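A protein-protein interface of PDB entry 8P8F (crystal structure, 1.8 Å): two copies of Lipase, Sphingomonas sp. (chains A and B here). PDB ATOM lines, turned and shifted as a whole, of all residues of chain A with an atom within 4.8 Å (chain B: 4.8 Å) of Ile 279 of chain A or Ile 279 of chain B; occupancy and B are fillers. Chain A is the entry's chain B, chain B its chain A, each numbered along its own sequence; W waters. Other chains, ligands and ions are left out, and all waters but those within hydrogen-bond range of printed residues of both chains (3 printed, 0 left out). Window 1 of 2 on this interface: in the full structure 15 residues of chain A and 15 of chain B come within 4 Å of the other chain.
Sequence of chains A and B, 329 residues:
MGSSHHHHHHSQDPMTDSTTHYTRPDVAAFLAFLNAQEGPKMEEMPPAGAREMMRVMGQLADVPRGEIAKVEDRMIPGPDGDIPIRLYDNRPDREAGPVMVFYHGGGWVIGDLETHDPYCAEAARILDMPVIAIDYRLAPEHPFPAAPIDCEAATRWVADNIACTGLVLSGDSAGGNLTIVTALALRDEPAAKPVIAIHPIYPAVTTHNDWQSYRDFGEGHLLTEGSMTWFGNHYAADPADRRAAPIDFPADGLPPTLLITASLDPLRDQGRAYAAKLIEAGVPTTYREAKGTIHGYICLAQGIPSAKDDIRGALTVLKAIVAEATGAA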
ATOM      1  N   ARG A 272      -0.822  21.449 -13.170  1.00  0.00           N
ATOM      2  CA  ARG A 272      -1.796  22.515 -12.977  1.00  0.00           C
ATOM      3  C   ARG A 272      -3.190  22.010 -13.308  1.00  0.00           C
ATOM      4  O   ARG A 272      -4.147  22.304 -12.589  1.00  0.00           O
ATOM      5  CB  ARG A 272      -1.455  23.769 -13.782  1.00  0.00           C
ATOM      6  CG  ARG A 272      -0.161  24.463 -13.394  1.00  0.00           C
ATOM      7  CD  ARG A 272       0.104  25.537 -14.455  1.00  0.00           C
ATOM      8  NE  ARG A 272       1.245  26.406 -14.168  1.00  0.00           N
ATOM      9  CZ  ARG A 272       1.587  27.456 -14.913  1.00  0.00           C
ATOM     10  NH1 ARG A 272       0.993  27.661 -16.072  1.00  0.00           N
ATOM     11  NH2 ARG A 272       2.609  28.238 -14.569  1.00  0.00           N
ATOM     12  N   ALA A 275      -4.670  19.753 -10.576  1.00  0.00           N
ATOM     13  CA  ALA A 275      -5.013  20.517  -9.379  1.00  0.00           C
ATOM     14  C   ALA A 275      -6.334  21.285  -9.604  1.00  0.00           C
ATOM     15  O   ALA A 275      -7.226  21.347  -8.733  1.00  0.00           O
ATOM     16  CB  ALA A 275      -3.871  21.423  -9.022  1.00  0.00           C
ATOM     17  N   ALA A 276      -6.499  21.837 -10.811  1.00  0.00           N
ATOM     18  CA  ALA A 276      -7.687  22.573 -11.167  1.00  0.00           C
ATOM     19  C   ALA A 276      -8.899  21.638 -11.220  1.00  0.00           C
ATOM     20  O   ALA A 276      -9.992  21.972 -10.748  1.00  0.00           O
ATOM     21  CB  ALA A 276      -7.498  23.282 -12.474  1.00  0.00           C
ATOM     22  N   LYS A 277      -8.699  20.421 -11.731  1.00  0.00           N
ATOM     23  CA  LYS A 277      -9.742  19.425 -11.747  1.00  0.00           C
ATOM     24  C   LYS A 277     -10.191  19.041 -10.328  1.00  0.00           C
ATOM     25  O   LYS A 277     -11.380  18.850 -10.098  1.00  0.00           O
ATOM     26  CB  LYS A 277      -9.199  18.202 -12.473  1.00  0.00           C
ATOM     27  CG  LYS A 277     -10.175  17.051 -12.627  1.00  0.00           C
ATOM     28  CD  LYS A 277      -9.427  15.873 -13.269  1.00  0.00           C
ATOM     29  CE  LYS A 277     -10.196  14.582 -13.335  1.00  0.00           C
ATOM     30  NZ  LYS A 277     -11.370  14.754 -14.221  1.00  0.00           N
ATOM     31  N   LEU A 278      -9.257  18.857  -9.417  1.00  0.00           N
ATOM     32  CA  LEU A 278      -9.596  18.559  -8.025  1.00  0.00           C
ATOM     33  C   LEU A 278     -10.490  19.645  -7.429  1.00  0.00           C
ATOM     34  O   LEU A 278     -11.496  19.326  -6.760  1.00  0.00           O
ATOM     35  CB  LEU A 278      -8.312  18.423  -7.211  1.00  0.00           C
ATOM     36  CG  LEU A 278      -7.493  17.173  -7.485  1.00  0.00           C
ATOM     37  CD1 LEU A 278      -6.111  17.219  -6.839  1.00  0.00           C
ATOM     38  CD2 LEU A 278      -8.253  16.012  -6.959  1.00  0.00           C
ATOM     39  N   ILE A 279     -10.140  20.913  -7.684  1.00  0.00           N
ATOM     40  CA  ILE A 279     -10.902  22.015  -7.158  1.00  0.00           C
ATOM     41  C   ILE A 279     -12.322  21.985  -7.717  1.00  0.00           C
ATOM     42  O   ILE A 279     -13.303  22.119  -6.986  1.00  0.00           O
ATOM     43  CB  ILE A 279     -10.141  23.317  -7.379  1.00  0.00           C
ATOM     44  CG1 ILE A 279      -8.873  23.349  -6.501  1.00  0.00           C
ATOM     45  CG2 ILE A 279     -10.997  24.502  -7.146  1.00  0.00           C
ATOM     46  CD1 ILE A 279      -8.005  24.565  -6.708  1.00  0.00           C
ATOM     47  N   GLU A 280     -12.439  21.821  -9.045  1.00  0.00           N
ATOM     48  CA  GLU A 280     -13.731  21.755  -9.685  1.00  0.00           C
ATOM     49  C   GLU A 280     -14.606  20.640  -9.132  1.00  0.00           C
ATOM     50  O   GLU A 280     -15.867  20.701  -9.226  1.00  0.00           O
ATOM     51  CB  GLU A 280     -13.475  21.701 -11.188  1.00  0.00           C
ATOM     52  CG  GLU A 280     -13.152  23.119 -11.708  1.00  0.00           C
ATOM     53  CD  GLU A 280     -12.713  23.255 -13.167  1.00  0.00           C
ATOM     54  OE1 GLU A 280     -11.964  22.357 -13.668  1.00  0.00           O
ATOM     55  OE2 GLU A 280     -13.096  24.285 -13.795  1.00  0.00           O
ATOM     56  N   ALA A 281     -13.962  19.558  -8.679  1.00  0.00           N
ATOM     57  CA  ALA A 281     -14.655  18.445  -8.049  1.00  0.00           C
ATOM     58  C   ALA A 281     -14.899  18.668  -6.544  1.00  0.00           C
ATOM     59  O   ALA A 281     -15.331  17.757  -5.841  1.00  0.00           O
ATOM     60  CB  ALA A 281     -13.825  17.215  -8.249  1.00  0.00           C
ATOM     61  N   GLY A 282     -14.586  19.847  -6.012  1.00  0.00           N
ATOM     62  CA  GLY A 282     -14.776  20.117  -4.601  1.00  0.00           C
ATOM     63  C   GLY A 282     -13.784  19.465  -3.656  1.00  0.00           C
ATOM     64  O   GLY A 282     -14.062  19.398  -2.463  1.00  0.00           O
ATOM     65  N   VAL A 283     -12.600  19.047  -4.142  1.00  0.00           N
ATOM     66  CA  VAL A 283     -11.568  18.528  -3.248  1.00  0.00           C
ATOM     67  C   VAL A 283     -10.697  19.652  -2.704  1.00  0.00           C
ATOM     68  O   VAL A 283     -10.175  20.395  -3.490  1.00  0.00           O
ATOM     69  CB  VAL A 283     -10.689  17.479  -3.971  1.00  0.00           C
ATOM     70  CG1 VAL A 283      -9.567  16.940  -3.096  1.00  0.00           C
ATOM     71  CG2 VAL A 283     -11.533  16.326  -4.462  1.00  0.00           C
ATOM     72  N   THR A 285      -7.645  21.560  -1.863  1.00  0.00           N
ATOM     73  CA  THR A 285      -6.434  21.458  -2.689  1.00  0.00           C
ATOM     74  C   THR A 285      -5.513  22.610  -2.337  1.00  0.00           C
ATOM     75  O   THR A 285      -5.955  23.743  -2.380  1.00  0.00           O
ATOM     76  CB  THR A 285      -6.761  21.444  -4.212  1.00  0.00           C
ATOM     77  OG1 THR A 285      -7.665  20.371  -4.489  1.00  0.00           O
ATOM     78  CG2 THR A 285      -5.528  21.311  -5.107  1.00  0.00           C
ATOM     79  N   TYR A 287      -2.146  24.170  -4.040  1.00  0.00           N
ATOM     80  CA  TYR A 287      -1.306  24.138  -5.212  1.00  0.00           C
ATOM     81  C   TYR A 287      -0.080  24.984  -4.913  1.00  0.00           C
ATOM     82  O   TYR A 287      -0.196  26.210  -4.647  1.00  0.00           O
ATOM     83  CB  TYR A 287      -2.069  24.652  -6.408  1.00  0.00           C
ATOM     84  CG  TYR A 287      -1.157  24.682  -7.614  1.00  0.00           C
ATOM     85  CD1 TYR A 287      -0.703  23.518  -8.195  1.00  0.00           C
ATOM     86  CD2 TYR A 287      -0.671  25.869  -8.107  1.00  0.00           C
ATOM     87  CE1 TYR A 287       0.191  23.547  -9.254  1.00  0.00           C
ATOM     88  CE2 TYR A 287       0.215  25.911  -9.174  1.00  0.00           C
ATOM     89  CZ  TYR A 287       0.633  24.738  -9.748  1.00  0.00           C
ATOM     90  OH  TYR A 287       1.547  24.726 -10.764  1.00  0.00           O
ATOM     91  N   ARG B 272     -14.907  27.973  -7.082  1.00  0.00           N
ATOM     92  CA  ARG B 272     -14.112  26.865  -7.584  1.00  0.00           C
ATOM     93  C   ARG B 272     -13.518  27.229  -8.940  1.00  0.00           C
ATOM     94  O   ARG B 272     -12.340  26.965  -9.140  1.00  0.00           O
ATOM     95  CB  ARG B 272     -14.891  25.558  -7.747  1.00  0.00           C
ATOM     96  CG  ARG B 272     -15.393  24.959  -6.448  1.00  0.00           C
ATOM     97  CD  ARG B 272     -16.284  23.758  -6.783  1.00  0.00           C
ATOM     98  NE  ARG B 272     -16.803  23.024  -5.615  1.00  0.00           N
ATOM     99  CZ  ARG B 272     -17.678  22.000  -5.711  1.00  0.00           C
ATOM    100  NH1 ARG B 272     -18.191  21.627  -6.887  1.00  0.00           N
ATOM    101  NH2 ARG B 272     -17.990  21.295  -4.637  1.00  0.00           N
ATOM    102  N   ALA B 275     -10.600  29.701  -8.551  1.00  0.00           N
ATOM    103  CA  ALA B 275      -9.438  29.035  -7.976  1.00  0.00           C
ATOM    104  C   ALA B 275      -8.742  28.182  -9.029  1.00  0.00           C
ATOM    105  O   ALA B 275      -7.489  28.228  -9.188  1.00  0.00           O
ATOM    106  CB  ALA B 275      -9.846  28.246  -6.735  1.00  0.00           C
ATOM    107  N   ALA B 276      -9.537  27.471  -9.844  1.00  0.00           N
ATOM    108  CA  ALA B 276      -8.992  26.709 -10.945  1.00  0.00           C
ATOM    109  C   ALA B 276      -8.244  27.581 -11.953  1.00  0.00           C
ATOM    110  O   ALA B 276      -7.171  27.213 -12.420  1.00  0.00           O
ATOM    111  CB  ALA B 276     -10.094  25.903 -11.616  1.00  0.00           C
ATOM    112  N   LYS B 277      -8.808  28.753 -12.292  1.00  0.00           N
ATOM    113  CA  LYS B 277      -8.195  29.684 -13.215  1.00  0.00           C
ATOM    114  C   LYS B 277      -6.854  30.149 -12.706  1.00  0.00           C
ATOM    115  O   LYS B 277      -5.931  30.287 -13.473  1.00  0.00           O
ATOM    116  CB  LYS B 277      -9.160  30.845 -13.371  1.00  0.00           C
ATOM    117  CG  LYS B 277      -8.732  31.937 -14.345  1.00  0.00           C
ATOM    118  CD  LYS B 277      -9.799  33.017 -14.386  1.00  0.00           C
ATOM    119  CE  LYS B 277      -9.370  34.255 -15.144  1.00  0.00           C
ATOM    120  NZ  LYS B 277      -9.231  33.944 -16.594  1.00  0.00           N
ATOM    121  N   LEU B 278      -6.771  30.477 -11.417  1.00  0.00           N
ATOM    122  CA  LEU B 278      -5.553  30.941 -10.815  1.00  0.00           C
ATOM    123  C   LEU B 278      -4.462  29.890 -10.977  1.00  0.00           C
ATOM    124  O   LEU B 278      -3.338  30.232 -11.340  1.00  0.00           O
ATOM    125  CB  LEU B 278      -5.821  31.230  -9.316  1.00  0.00           C
ATOM    126  CG  LEU B 278      -6.555  32.504  -8.999  1.00  0.00           C
ATOM    127  CD1 LEU B 278      -6.949  32.553  -7.535  1.00  0.00           C
ATOM    128  CD2 LEU B 278      -5.711  33.704  -9.330  1.00  0.00           C
ATOM    129  N   ILE B 279      -4.800  28.635 -10.704  1.00  0.00           N
ATOM    130  CA  ILE B 279      -3.813  27.551 -10.838  1.00  0.00           C
ATOM    131  C   ILE B 279      -3.326  27.399 -12.249  1.00  0.00           C
ATOM    132  O   ILE B 279      -2.090  27.325 -12.485  1.00  0.00           O
ATOM    133  CB  ILE B 279      -4.444  26.285 -10.277  1.00  0.00           C
ATOM    134  CG1 ILE B 279      -4.593  26.476  -8.742  1.00  0.00           C
ATOM    135  CG2 ILE B 279      -3.653  25.056 -10.657  1.00  0.00           C
ATOM    136  CD1 ILE B 279      -5.221  25.301  -8.028  1.00  0.00           C
ATOM    137  N   GLU B 280      -4.295  27.411 -13.153  1.00  0.00           N
ATOM    138  CA  GLU B 280      -3.966  27.329 -14.580  1.00  0.00           C
ATOM    139  C   GLU B 280      -3.103  28.499 -15.059  1.00  0.00           C
ATOM    140  O   GLU B 280      -2.389  28.357 -16.085  1.00  0.00           O
ATOM    141  CB  GLU B 280      -5.280  27.135 -15.345  1.00  0.00           C
ATOM    142  CG  GLU B 280      -5.713  25.688 -15.179  1.00  0.00           C
ATOM    143  CD  GLU B 280      -7.021  25.144 -15.747  1.00  0.00           C
ATOM    144  OE1 GLU B 280      -8.085  25.791 -15.515  1.00  0.00           O
ATOM    145  OE2 GLU B 280      -6.987  23.976 -16.335  1.00  0.00           O
ATOM    146  N   ALA B 281      -3.131  29.614 -14.345  1.00  0.00           N
ATOM    147  CA  ALA B 281      -2.237  30.746 -14.586  1.00  0.00           C
ATOM    148  C   ALA B 281      -0.950  30.716 -13.785  1.00  0.00           C
ATOM    149  O   ALA B 281      -0.207  31.684 -13.806  1.00  0.00           O
ATOM    150  CB  ALA B 281      -2.929  32.025 -14.335  1.00  0.00           C
ATOM    151  N   GLY B 282      -0.679  29.662 -13.041  1.00  0.00           N
ATOM    152  CA  GLY B 282       0.582  29.558 -12.321  1.00  0.00           C
ATOM    153  C   GLY B 282       0.568  30.327 -10.994  1.00  0.00           C
ATOM    154  O   GLY B 282       1.631  30.564 -10.409  1.00  0.00           O
ATOM    155  N   VAL B 283      -0.604  30.732 -10.509  1.00  0.00           N
ATOM    156  CA  VAL B 283      -0.684  31.399  -9.226  1.00  0.00           C
ATOM    157  C   VAL B 283      -0.761  30.390  -8.081  1.00  0.00           C
ATOM    158  O   VAL B 283      -1.658  29.560  -8.093  1.00  0.00           O
ATOM    159  CB  VAL B 283      -1.870  32.368  -9.145  1.00  0.00           C
ATOM    160  CG1 VAL B 283      -1.953  33.078  -7.822  1.00  0.00           C
ATOM    161  CG2 VAL B 283      -1.833  33.387 -10.257  1.00  0.00           C
ATOM    162  N   THR B 285      -1.983  28.787  -4.957  1.00  0.00           N
ATOM    163  CA  THR B 285      -3.434  28.866  -4.620  1.00  0.00           C
ATOM    164  C   THR B 285      -3.748  27.771  -3.628  1.00  0.00           C
ATOM    165  O   THR B 285      -3.500  26.577  -3.889  1.00  0.00           O
ATOM    166  CB  THR B 285      -4.356  28.710  -5.841  1.00  0.00           C
ATOM    167  OG1 THR B 285      -4.070  29.690  -6.813  1.00  0.00           O
ATOM    168  CG2 THR B 285      -5.841  28.792  -5.557  1.00  0.00           C
ATOM    169  N   TYR B 287      -7.068  26.202  -1.907  1.00  0.00           N
ATOM    170  CA  TYR B 287      -8.526  26.148  -2.020  1.00  0.00           C
ATOM    171  C   TYR B 287      -9.052  25.423  -0.821  1.00  0.00           C
ATOM    172  O   TYR B 287      -8.650  24.281  -0.600  1.00  0.00           O
ATOM    173  CB  TYR B 287      -8.898  25.530  -3.347  1.00  0.00           C
ATOM    174  CG  TYR B 287     -10.394  25.335  -3.412  1.00  0.00           C
ATOM    175  CD1 TYR B 287     -11.180  26.433  -3.569  1.00  0.00           C
ATOM    176  CD2 TYR B 287     -10.998  24.129  -3.184  1.00  0.00           C
ATOM    177  CE1 TYR B 287     -12.566  26.355  -3.599  1.00  0.00           C
ATOM    178  CE2 TYR B 287     -12.384  24.026  -3.216  1.00  0.00           C
ATOM    179  CZ  TYR B 287     -13.154  25.153  -3.429  1.00  0.00           C
ATOM    180  OH  TYR B 287     -14.557  25.133  -3.418  1.00  0.00           O
HETATM  181  O   HOH W   1      -1.411  26.200 -17.576  1.00  0.00           O
HETATM  182  O   HOH W   2     -17.655  22.761  -9.672  1.00  0.00           O
HETATM  183  O   HOH W   3      -0.164  27.423  -2.407  1.00  0.00           O
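The backbone NH of Tyr 287 of chain B lies within hydrogen-bond range of the backbone carbonyl oxygen of Thr 285 of chain A (2.7 Å). O of Thr 285 of chain B is in hydrogen-bond range of N of Tyr 287 of chain A (2.8 Å). The guanidinium group (NH1) of Arg 272 of chain A lies within hydrogen-bond range of the backbone carbonyl oxygen (O) of Glu 280 of chain B, 3.5 Å away. The backbone carbonyl oxygen (O) of Glu 280 of chain A sits at hydrogen-bond distance from the guanidinium group (NH1) of Arg 272 of chain B.
The backbone carbonyl oxygen (O) of Val 283 of chain B sits at hydrogen-bond distance from the side-chain hydroxyl (OG1) of Thr 285 of chain B, at 2.7 Å. The side-chain hydroxyl of Thr 285 of chain A lies within hydrogen-bond range of the backbone carbonyl oxygen of Val 283 of chain A, at 2.7 Å. The backbone NH (N) of Val 283 of chain B sits at hydrogen-bond distance from the backbone carbonyl oxygen (O) of Leu 278 of chain B, at 2.9 Å. The backbone NH (N) of Val 283 of chain A is in hydrogen-bond range of the backbone carbonyl oxygen (O) of Leu 278 of chain A (2.9 Å).
Gly 282 of chain B touches Arg 272 of chain A. Ile 279 of chain B touches Ala 275 of chain A (CG2 to CB, 3.99 Å). Ala 276 of chain A touches Ala 276 of chain B (CB to CB, 3.8 Å). O of Ile 279 of chain A touches CD of Arg 272 of chain B, at 3.4 Å. CB of Ala 275 of chain B touches CG2 of Ile 279 of chain A, at 3.9 Å. Ile 279 of chain B touches Ile 279 of chain A (CD1 to CD1, 3.2 Å). CD1 of Ile 279 of chain A touches CB of Tyr 287 of chain B, at 3.6 Å. CA of Gly 282 of chain A touches NH2 of Arg 272 of chain B (3.4 Å). Val 283 of chain A touches Tyr 287 of chain B. CB of Tyr 287 of chain A touches CD1 of Ile 279 of chain B (3.6 Å).
Printed residues of chain B within 4 Å of Ala 275 of chain A: Ile 279 (3.99 Å). Ile 279 of chain A touches just these residues of chain B: Arg 272, Ala 275, Ile 279 and Tyr 287. Of the printed residues of chain B, Thr 285 of chain A touches Tyr 287. Printed residues of chain A within 4 Å of Ile 279 of chain B: Arg 272, Ala 275, Ile 279 and Tyr 287. The nearest printed residue of chain A that does not touch Ile 279 of chain B is Ala 276 of chain A (4.3 Å). The nearest printed residue of chain B that does not touch Thr 285 of chain A is Thr 285 of chain B (4.04 Å).
Of the 12 printed residues of chain B, 9 touch a printed residue of chain A. Printed residues of chain B that touch a printed residue of chain A: Arg 272, Ala 275, Ala 276, Ile 279, Glu 280, Gly 282, Val 283, Thr 285 and Tyr 287. Hydrophobic or aromatic side chains of chain B that line the printed part of chain A: Ala 275, Ala 276, Ile 279 and Tyr 287. Along chain A the printed residues that touch a printed residue of chain B span positions 272 to 287. Among the printed residues, 17 pairs touch across the chains. Among the printed residues, no Asp or Glu carboxylate lies within 4 Å of a Lys or Arg side-chain nitrogen of the other chain.
Arg 272 of chain A touches Gly 282 of chain B, and with the chains exchanged Gly 282 of chain A touches Arg 272 of chain B. Ala 276 of chain B touches its own counterpart, Ala 276 of chain A. Ala 276 of chain A touches Glu 280 of chain B, but with the chains exchanged Glu 280 of chain A does not touch Ala 276 of chain B (4.03 Å). Thr 285 of chain A touches Tyr 287 of chain B, and with the chains exchanged Tyr 287 of chain A touches Thr 285 of chain B. Of the 17 pairs that touch across the chains among the printed residues, 16 have their exchanged pair printed and touching as well.
Water W3 lies within hydrogen-bond range of O of Tyr 287 of chain A and N of Thr 285 of chain B. Water W2 bridges O of Glu 280 of chain A (2.8 Å) and NH1 of Arg 272 of chain B (3.1 Å). Water W1 lies within hydrogen-bond range of the backbone carbonyl oxygen (O) of Glu 280 of chain B (2.8 Å) and the guanidinium group (NH1) of Arg 272 of chain A (3.2 Å).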
